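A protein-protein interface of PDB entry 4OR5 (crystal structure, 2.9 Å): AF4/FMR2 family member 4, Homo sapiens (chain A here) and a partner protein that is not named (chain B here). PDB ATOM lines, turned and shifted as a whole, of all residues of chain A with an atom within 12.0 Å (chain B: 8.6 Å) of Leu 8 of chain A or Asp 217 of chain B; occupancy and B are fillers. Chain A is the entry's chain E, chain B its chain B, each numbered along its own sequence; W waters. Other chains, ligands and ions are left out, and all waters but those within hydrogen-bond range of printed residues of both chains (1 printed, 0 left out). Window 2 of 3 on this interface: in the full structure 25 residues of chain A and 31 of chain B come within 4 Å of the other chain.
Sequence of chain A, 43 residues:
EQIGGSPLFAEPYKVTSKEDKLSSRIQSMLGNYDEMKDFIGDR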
ATOM      1  N   SER A   6     -34.747   1.892  25.709  1.00  0.00           N
ATOM      2  CA  SER A   6     -33.579   2.606  26.312  1.00  0.00           C
ATOM      3  C   SER A   6     -33.089   3.723  25.376  1.00  0.00           C
ATOM      4  O   SER A   6     -33.296   3.654  24.160  1.00  0.00           O
ATOM      5  CB  SER A   6     -32.443   1.609  26.591  1.00  0.00           C
ATOM      6  OG  SER A   6     -32.057   0.911  25.417  1.00  0.00           O
ATOM      7  N   PRO A   7     -32.456   4.780  25.937  1.00  0.00           N
ATOM      8  CA  PRO A   7     -31.935   5.914  25.158  1.00  0.00           C
ATOM      9  C   PRO A   7     -30.765   5.518  24.262  1.00  0.00           C
ATOM     10  O   PRO A   7     -30.073   4.529  24.522  1.00  0.00           O
ATOM     11  CB  PRO A   7     -31.515   6.914  26.235  1.00  0.00           C
ATOM     12  CG  PRO A   7     -32.447   6.615  27.354  1.00  0.00           C
ATOM     13  CD  PRO A   7     -32.432   5.101  27.376  1.00  0.00           C
ATOM     14  N   LEU A   8     -30.539   6.307  23.215  1.00  0.00           N
ATOM     15  CA  LEU A   8     -29.470   6.034  22.265  1.00  0.00           C
ATOM     16  C   LEU A   8     -28.087   6.469  22.745  1.00  0.00           C
ATOM     17  O   LEU A   8     -27.059   5.940  22.312  1.00  0.00           O
ATOM     18  CB  LEU A   8     -29.794   6.713  20.939  1.00  0.00           C
ATOM     19  CG  LEU A   8     -28.782   6.490  19.825  1.00  0.00           C
ATOM     20  CD1 LEU A   8     -28.659   5.014  19.554  1.00  0.00           C
ATOM     21  CD2 LEU A   8     -29.228   7.218  18.582  1.00  0.00           C
ATOM     22  N   PHE A   9     -28.062   7.435  23.649  1.00  0.00           N
ATOM     23  CA  PHE A   9     -26.795   7.938  24.174  1.00  0.00           C
ATOM     24  C   PHE A   9     -26.746   7.973  25.703  1.00  0.00           C
ATOM     25  O   PHE A   9     -27.687   8.433  26.363  1.00  0.00           O
ATOM     26  CB  PHE A   9     -26.522   9.356  23.624  1.00  0.00           C
ATOM     27  CG  PHE A   9     -25.692   9.383  22.363  1.00  0.00           C
ATOM     28  CD1 PHE A   9     -24.304   9.213  22.425  1.00  0.00           C
ATOM     29  CD2 PHE A   9     -26.298   9.553  21.109  1.00  0.00           C
ATOM     30  CE1 PHE A   9     -23.527   9.207  21.257  1.00  0.00           C
ATOM     31  CE2 PHE A   9     -25.533   9.549  19.937  1.00  0.00           C
ATOM     32  CZ  PHE A   9     -24.144   9.374  20.011  1.00  0.00           C
ATOM     33  N   ALA A  10     -25.649   7.474  26.265  1.00  0.00           N
ATOM     34  CA  ALA A  10     -25.476   7.514  27.714  1.00  0.00           C
ATOM     35  C   ALA A  10     -25.271   8.993  27.972  1.00  0.00           C
ATOM     36  O   ALA A  10     -25.144   9.773  27.034  1.00  0.00           O
ATOM     37  CB  ALA A  10     -24.232   6.729  28.139  1.00  0.00           C
ATOM     38  N   GLU A  11     -25.227   9.393  29.228  1.00  0.00           N
ATOM     39  CA  GLU A  11     -25.028  10.802  29.537  1.00  0.00           C
ATOM     40  C   GLU A  11     -23.534  11.157  29.520  1.00  0.00           C
ATOM     41  O   GLU A  11     -22.689  10.344  29.878  1.00  0.00           O
ATOM     42  CB  GLU A  11     -25.646  11.119  30.910  1.00  0.00           C
ATOM     43  CG  GLU A  11     -26.850  12.082  30.888  1.00  0.00           C
ATOM     44  CD  GLU A  11     -27.609  12.159  32.230  1.00  0.00           C
ATOM     45  OE1 GLU A  11     -26.960  12.163  33.297  1.00  0.00           O
ATOM     46  OE2 GLU A  11     -28.859  12.233  32.216  1.00  0.00           O
ATOM     47  N   PRO A  12     -23.195  12.380  29.085  1.00  0.00           N
ATOM     48  CA  PRO A  12     -21.812  12.871  29.015  1.00  0.00           C
ATOM     49  C   PRO A  12     -21.124  12.738  30.367  1.00  0.00           C
ATOM     50  O   PRO A  12     -21.717  13.050  31.402  1.00  0.00           O
ATOM     51  CB  PRO A  12     -21.984  14.334  28.626  1.00  0.00           C
ATOM     52  CG  PRO A  12     -23.251  14.322  27.828  1.00  0.00           C
ATOM     53  CD  PRO A  12     -24.140  13.402  28.607  1.00  0.00           C
ATOM     54  N   TYR A  13     -19.872  12.306  30.360  1.00  0.00           N
ATOM     55  CA  TYR A  13     -19.148  12.122  31.610  1.00  0.00           C
ATOM     56  C   TYR A  13     -17.828  12.886  31.687  1.00  0.00           C
ATOM     57  O   TYR A  13     -17.058  12.875  30.738  1.00  0.00           O
ATOM     58  CB  TYR A  13     -18.879  10.638  31.814  1.00  0.00           C
ATOM     59  CG  TYR A  13     -18.069  10.030  30.703  1.00  0.00           C
ATOM     60  CD1 TYR A  13     -18.683   9.535  29.553  1.00  0.00           C
ATOM     61  CD2 TYR A  13     -16.678   9.973  30.791  1.00  0.00           C
ATOM     62  CE1 TYR A  13     -17.927   8.990  28.503  1.00  0.00           C
ATOM     63  CE2 TYR A  13     -15.914   9.438  29.762  1.00  0.00           C
ATOM     64  CZ  TYR A  13     -16.537   8.950  28.617  1.00  0.00           C
ATOM     65  OH  TYR A  13     -15.754   8.463  27.588  1.00  0.00           O
ATOM     66  N   LEU B 163     -29.688  15.319  21.169  1.00  0.00           N
ATOM     67  CA  LEU B 163     -29.568  13.887  20.948  1.00  0.00           C
ATOM     68  C   LEU B 163     -28.483  13.227  21.816  1.00  0.00           C
ATOM     69  O   LEU B 163     -28.486  12.015  21.997  1.00  0.00           O
ATOM     70  CB  LEU B 163     -29.337  13.600  19.458  1.00  0.00           C
ATOM     71  CG  LEU B 163     -28.905  12.186  19.045  1.00  0.00           C
ATOM     72  CD1 LEU B 163     -29.404  11.864  17.640  1.00  0.00           C
ATOM     73  CD2 LEU B 163     -27.383  12.085  19.120  1.00  0.00           C
ATOM     74  N   VAL B 164     -27.560  13.999  22.365  1.00  0.00           N
ATOM     75  CA  VAL B 164     -26.537  13.394  23.207  1.00  0.00           C
ATOM     76  C   VAL B 164     -26.748  13.756  24.678  1.00  0.00           C
ATOM     77  O   VAL B 164     -25.802  13.737  25.477  1.00  0.00           O
ATOM     78  CB  VAL B 164     -25.112  13.825  22.799  1.00  0.00           C
ATOM     79  CG1 VAL B 164     -24.694  13.114  21.539  1.00  0.00           C
ATOM     80  CG2 VAL B 164     -25.063  15.341  22.630  1.00  0.00           C
ATOM     81  N   ARG B 165     -27.987  14.092  25.025  1.00  0.00           N
ATOM     82  CA  ARG B 165     -28.327  14.443  26.401  1.00  0.00           C
ATOM     83  C   ARG B 165     -27.271  15.386  27.001  1.00  0.00           C
ATOM     84  O   ARG B 165     -26.907  15.280  28.174  1.00  0.00           O
ATOM     85  CB  ARG B 165     -28.428  13.171  27.268  1.00  0.00           C
ATOM     86  CG  ARG B 165     -29.398  12.074  26.784  1.00  0.00           C
ATOM     87  CD  ARG B 165     -29.443  10.892  27.782  1.00  0.00           C
ATOM     88  NE  ARG B 165     -30.623  10.908  28.654  1.00  0.00           N
ATOM     89  CZ  ARG B 165     -30.991  11.925  29.440  1.00  0.00           C
ATOM     90  NH1 ARG B 165     -30.277  13.046  29.490  1.00  0.00           N
ATOM     91  NH2 ARG B 165     -32.086  11.827  30.184  1.00  0.00           N
ATOM     92  N   ILE B 212     -18.520  12.485  25.227  1.00  0.00           N
ATOM     93  CA  ILE B 212     -19.763  11.919  24.733  1.00  0.00           C
ATOM     94  C   ILE B 212     -19.462  10.476  24.360  1.00  0.00           C
ATOM     95  O   ILE B 212     -18.710  10.206  23.431  1.00  0.00           O
ATOM     96  CB  ILE B 212     -20.284  12.711  23.529  1.00  0.00           C
ATOM     97  CG1 ILE B 212     -20.291  14.200  23.888  1.00  0.00           C
ATOM     98  CG2 ILE B 212     -21.692  12.253  23.166  1.00  0.00           C
ATOM     99  CD1 ILE B 212     -20.800  15.121  22.813  1.00  0.00           C
ATOM    100  N   PRO B 213     -20.031   9.525  25.114  1.00  0.00           N
ATOM    101  CA  PRO B 213     -19.845   8.090  24.902  1.00  0.00           C
ATOM    102  C   PRO B 213     -20.307   7.656  23.523  1.00  0.00           C
ATOM    103  O   PRO B 213     -21.126   8.330  22.889  1.00  0.00           O
ATOM    104  CB  PRO B 213     -20.692   7.478  26.010  1.00  0.00           C
ATOM    105  CG  PRO B 213     -21.833   8.451  26.103  1.00  0.00           C
ATOM    106  CD  PRO B 213     -21.113   9.771  26.086  1.00  0.00           C
ATOM    107  N   VAL B 214     -19.783   6.536  23.050  1.00  0.00           N
ATOM    108  CA  VAL B 214     -20.195   6.068  21.750  1.00  0.00           C
ATOM    109  C   VAL B 214     -21.659   5.683  21.824  1.00  0.00           C
ATOM    110  O   VAL B 214     -22.172   5.376  22.898  1.00  0.00           O
ATOM    111  CB  VAL B 214     -19.396   4.874  21.316  1.00  0.00           C
ATOM    112  CG1 VAL B 214     -19.762   4.531  19.891  1.00  0.00           C
ATOM    113  CG2 VAL B 214     -17.917   5.178  21.443  1.00  0.00           C
ATOM    114  N   SER B 215     -22.337   5.706  20.684  1.00  0.00           N
ATOM    115  CA  SER B 215     -23.751   5.371  20.642  1.00  0.00           C
ATOM    116  C   SER B 215     -23.954   3.899  20.968  1.00  0.00           C
ATOM    117  O   SER B 215     -23.046   3.086  20.780  1.00  0.00           O
ATOM    118  CB  SER B 215     -24.311   5.673  19.254  1.00  0.00           C
ATOM    119  OG  SER B 215     -25.720   5.598  19.264  1.00  0.00           O
ATOM    120  N   THR B 216     -25.139   3.548  21.461  1.00  0.00           N
ATOM    121  CA  THR B 216     -25.423   2.153  21.775  1.00  0.00           C
ATOM    122  C   THR B 216     -25.395   1.321  20.484  1.00  0.00           C
ATOM    123  O   THR B 216     -25.589   0.105  20.527  1.00  0.00           O
ATOM    124  CB  THR B 216     -26.806   1.964  22.492  1.00  0.00           C
ATOM    125  OG1 THR B 216     -27.882   2.331  21.617  1.00  0.00           O
ATOM    126  CG2 THR B 216     -26.868   2.813  23.756  1.00  0.00           C
ATOM    127  N   ASP B 217     -25.162   1.973  19.340  1.00  0.00           N
ATOM    128  CA  ASP B 217     -25.077   1.259  18.068  1.00  0.00           C
ATOM    129  C   ASP B 217     -23.672   1.274  17.524  1.00  0.00           C
ATOM    130  O   ASP B 217     -23.421   0.790  16.420  1.00  0.00           O
ATOM    131  CB  ASP B 217     -26.034   1.833  17.041  1.00  0.00           C
ATOM    132  CG  ASP B 217     -27.467   1.501  17.362  1.00  0.00           C
ATOM    133  OD1 ASP B 217     -28.259   1.235  16.427  1.00  0.00           O
ATOM    134  OD2 ASP B 217     -27.803   1.502  18.567  1.00  0.00           O
ATOM    135  N   GLY B 218     -22.760   1.836  18.314  1.00  0.00           N
ATOM    136  CA  GLY B 218     -21.359   1.888  17.939  1.00  0.00           C
ATOM    137  C   GLY B 218     -20.856   3.145  17.258  1.00  0.00           C
ATOM    138  O   GLY B 218     -19.657   3.430  17.295  1.00  0.00           O
ATOM    139  N   LYS B 219     -21.753   3.902  16.639  1.00  0.00           N
ATOM    140  CA  LYS B 219     -21.343   5.107  15.942  1.00  0.00           C
ATOM    141  C   LYS B 219     -20.936   6.233  16.917  1.00  0.00           C
ATOM    142  O   LYS B 219     -21.496   6.350  18.009  1.00  0.00           O
ATOM    143  CB  LYS B 219     -22.482   5.556  15.014  1.00  0.00           C
ATOM    144  CG  LYS B 219     -23.030   4.446  14.091  1.00  0.00           C
ATOM    145  CD  LYS B 219     -23.618   5.001  12.769  1.00  0.00           C
ATOM    146  CE  LYS B 219     -24.792   5.976  12.981  1.00  0.00           C
ATOM    147  NZ  LYS B 219     -25.196   6.717  11.736  1.00  0.00           N
ATOM    148  N   HIS B 220     -19.936   7.029  16.533  1.00  0.00           N
ATOM    149  CA  HIS B 220     -19.483   8.162  17.342  1.00  0.00           C
ATOM    150  C   HIS B 220     -20.584   9.225  17.337  1.00  0.00           C
ATOM    151  O   HIS B 220     -21.441   9.222  16.453  1.00  0.00           O
ATOM    152  CB  HIS B 220     -18.228   8.762  16.740  1.00  0.00           C
ATOM    153  CG  HIS B 220     -16.981   8.010  17.064  1.00  0.00           C
ATOM    154  ND1 HIS B 220     -16.407   8.033  18.318  1.00  0.00           N
ATOM    155  CD2 HIS B 220     -16.169   7.254  16.288  1.00  0.00           C
ATOM    156  CE1 HIS B 220     -15.288   7.329  18.297  1.00  0.00           C
ATOM    157  NE2 HIS B 220     -15.121   6.847  17.078  1.00  0.00           N
ATOM    158  N   TRP B 221     -20.561  10.156  18.288  1.00  0.00           N
ATOM    159  CA  TRP B 221     -21.625  11.159  18.330  1.00  0.00           C
ATOM    160  C   TRP B 221     -21.774  11.969  17.049  1.00  0.00           C
ATOM    161  O   TRP B 221     -22.897  12.140  16.551  1.00  0.00           O
ATOM    162  CB  TRP B 221     -21.482  12.108  19.553  1.00  0.00           C
ATOM    163  CG  TRP B 221     -20.255  13.000  19.597  1.00  0.00           C
ATOM    164  CD1 TRP B 221     -19.075  12.757  20.259  1.00  0.00           C
ATOM    165  CD2 TRP B 221     -20.093  14.273  18.952  1.00  0.00           C
ATOM    166  NE1 TRP B 221     -18.196  13.797  20.065  1.00  0.00           N
ATOM    167  CE2 TRP B 221     -18.795  14.740  19.266  1.00  0.00           C
ATOM    168  CE3 TRP B 221     -20.922  15.067  18.136  1.00  0.00           C
ATOM    169  CZ2 TRP B 221     -18.307  15.965  18.792  1.00  0.00           C
ATOM    170  CZ3 TRP B 221     -20.435  16.291  17.664  1.00  0.00           C
ATOM    171  CH2 TRP B 221     -19.142  16.723  17.994  1.00  0.00           C
ATOM    172  N   GLU B 223     -21.097  11.212  14.031  1.00  0.00           N
ATOM    173  CA  GLU B 223     -21.616  10.448  12.901  1.00  0.00           C
ATOM    174  C   GLU B 223     -23.128  10.601  12.784  1.00  0.00           C
ATOM    175  O   GLU B 223     -23.733  10.084  11.853  1.00  0.00           O
ATOM    176  CB  GLU B 223     -21.289   8.966  13.049  1.00  0.00           C
ATOM    177  CG  GLU B 223     -19.851   8.670  13.437  1.00  0.00           C
ATOM    178  CD  GLU B 223     -19.470   7.217  13.178  1.00  0.00           C
ATOM    179  OE1 GLU B 223     -18.732   6.630  14.006  1.00  0.00           O
ATOM    180  OE2 GLU B 223     -19.900   6.670  12.136  1.00  0.00           O
ATOM    181  N   TYR B 224     -23.739  11.297  13.739  1.00  0.00           N
ATOM    182  CA  TYR B 224     -25.182  11.517  13.723  1.00  0.00           C
ATOM    183  C   TYR B 224     -25.461  12.938  13.288  1.00  0.00           C
ATOM    184  O   TYR B 224     -26.623  13.335  13.190  1.00  0.00           O
ATOM    185  CB  TYR B 224     -25.810  11.299  15.114  1.00  0.00           C
ATOM    186  CG  TYR B 224     -25.839   9.861  15.561  1.00  0.00           C
ATOM    187  CD1 TYR B 224     -24.717   9.267  16.145  1.00  0.00           C
ATOM    188  CD2 TYR B 224     -26.963   9.066  15.328  1.00  0.00           C
ATOM    189  CE1 TYR B 224     -24.713   7.909  16.479  1.00  0.00           C
ATOM    190  CE2 TYR B 224     -26.972   7.708  15.653  1.00  0.00           C
ATOM    191  CZ  TYR B 224     -25.845   7.134  16.224  1.00  0.00           C
ATOM    192  OH  TYR B 224     -25.836   5.784  16.506  1.00  0.00           O
HETATM  193  O   HOH W   1     -23.822  12.322  25.676  1.00  0.00           O
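The guanidinium group (NH1) of Arg 165 of chain B is in salt-bridge range of the side-chain carboxylate (OE2) of Glu 11 of chain A.
The side-chain hydroxyl of Ser 215 of chain B sits close to the backbone carbonyl oxygen of Leu 8 of chain A (3.3 Å).
The backbone NH (N) of Thr 216 of chain B lies within hydrogen-bond range of the backbone carbonyl oxygen (O) of Leu 8 of chain A.
OH of Tyr 224 of chain B lies within hydrogen-bond range of OG of Ser 215 of chain B, at 2.8 Å.
The side-chain hydroxyl of Thr 216 of chain B sits close to the side-chain carboxylate of Asp 217 of chain B, at 3.2 Å.
Thr 216 of chain B touches Pro 7 of chain A (CG2 to O, 3.7 Å).
CD1 of Leu 8 of chain A touches OD2 of Asp 217 of chain B (3.7 Å).
Leu 8 of chain A touches Tyr 224 of chain B (CD2 to CE2, 3.7 Å).
CD2 of Leu 163 of chain B touches CE2 of Phe 9 of chain A, 3.2 Å away.
CD2 of Phe 9 of chain A touches CG1 of Val 164 of chain B (3.9 Å).
CD of Arg 165 of chain B touches O of Phe 9 of chain A (3.3 Å).
CE1 of Phe 9 of chain A touches O of Pro 213 of chain B, 3.0 Å away.
Phe 9 of chain A touches Ser 215 of chain B (CE1 to N, 3.7 Å).
Phe 9 of chain A touches Trp 221 of chain B.
Val 164 of chain B touches Pro 12 of chain A (O to CG, 3.5 Å).
Of chain B, only Ser 215, Thr 216, Asp 217 and Tyr 224 come within 4 Å of Leu 8 of chain A.
Of chain A, only Leu 8 comes within 4 Å of Asp 217 of chain B.
Ser 215 of chain B touches just these residues of chain A: Leu 8 and Phe 9.
Of chain A, only Pro 7 (3.7 Å) and Leu 8 (3.2 Å) come within 4 Å of Thr 216 of chain B.
No residue of chain A comes within 4 Å of Gly 218 of chain B.
No residue of chain A comes within 4 Å of Lys 219 of chain B.
Of the printed residues of chain B, Ala 10 of chain A touches Pro 213.
Printed residues of chain A within 4 Å of Arg 165 of chain B: Phe 9, Glu 11 and Pro 12.
Tyr 13 of chain A touches none of the printed residues of chain B.
Ser 6 of chain A touches none of the printed residues of chain B.
The nearest residue of chain B that does not touch Leu 8 of chain A is Leu 163 of chain B (4.7 Å).
The nearest residue of chain A that does not touch Asp 217 of chain B is Pro 7 of chain A (7.1 Å).
Of the 15 printed residues of chain B, 9 touch a printed residue of chain A.
Hydrophobic or aromatic side chains of chain B that line the printed part of chain A: Leu 163, Val 164, Pro 213, Trp 221 and Tyr 224.
Of the 8 printed residues of chain A, 6 touch a printed residue of chain B.
Hydrophobic or aromatic side chains of chain A that line the printed part of chain B: Leu 8, Phe 9, Ala 10 and Pro 12.
Water W1 bridges O of Val 164 of chain B (2.4 Å) and O of Ala 10 of chain A (3.2 Å).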
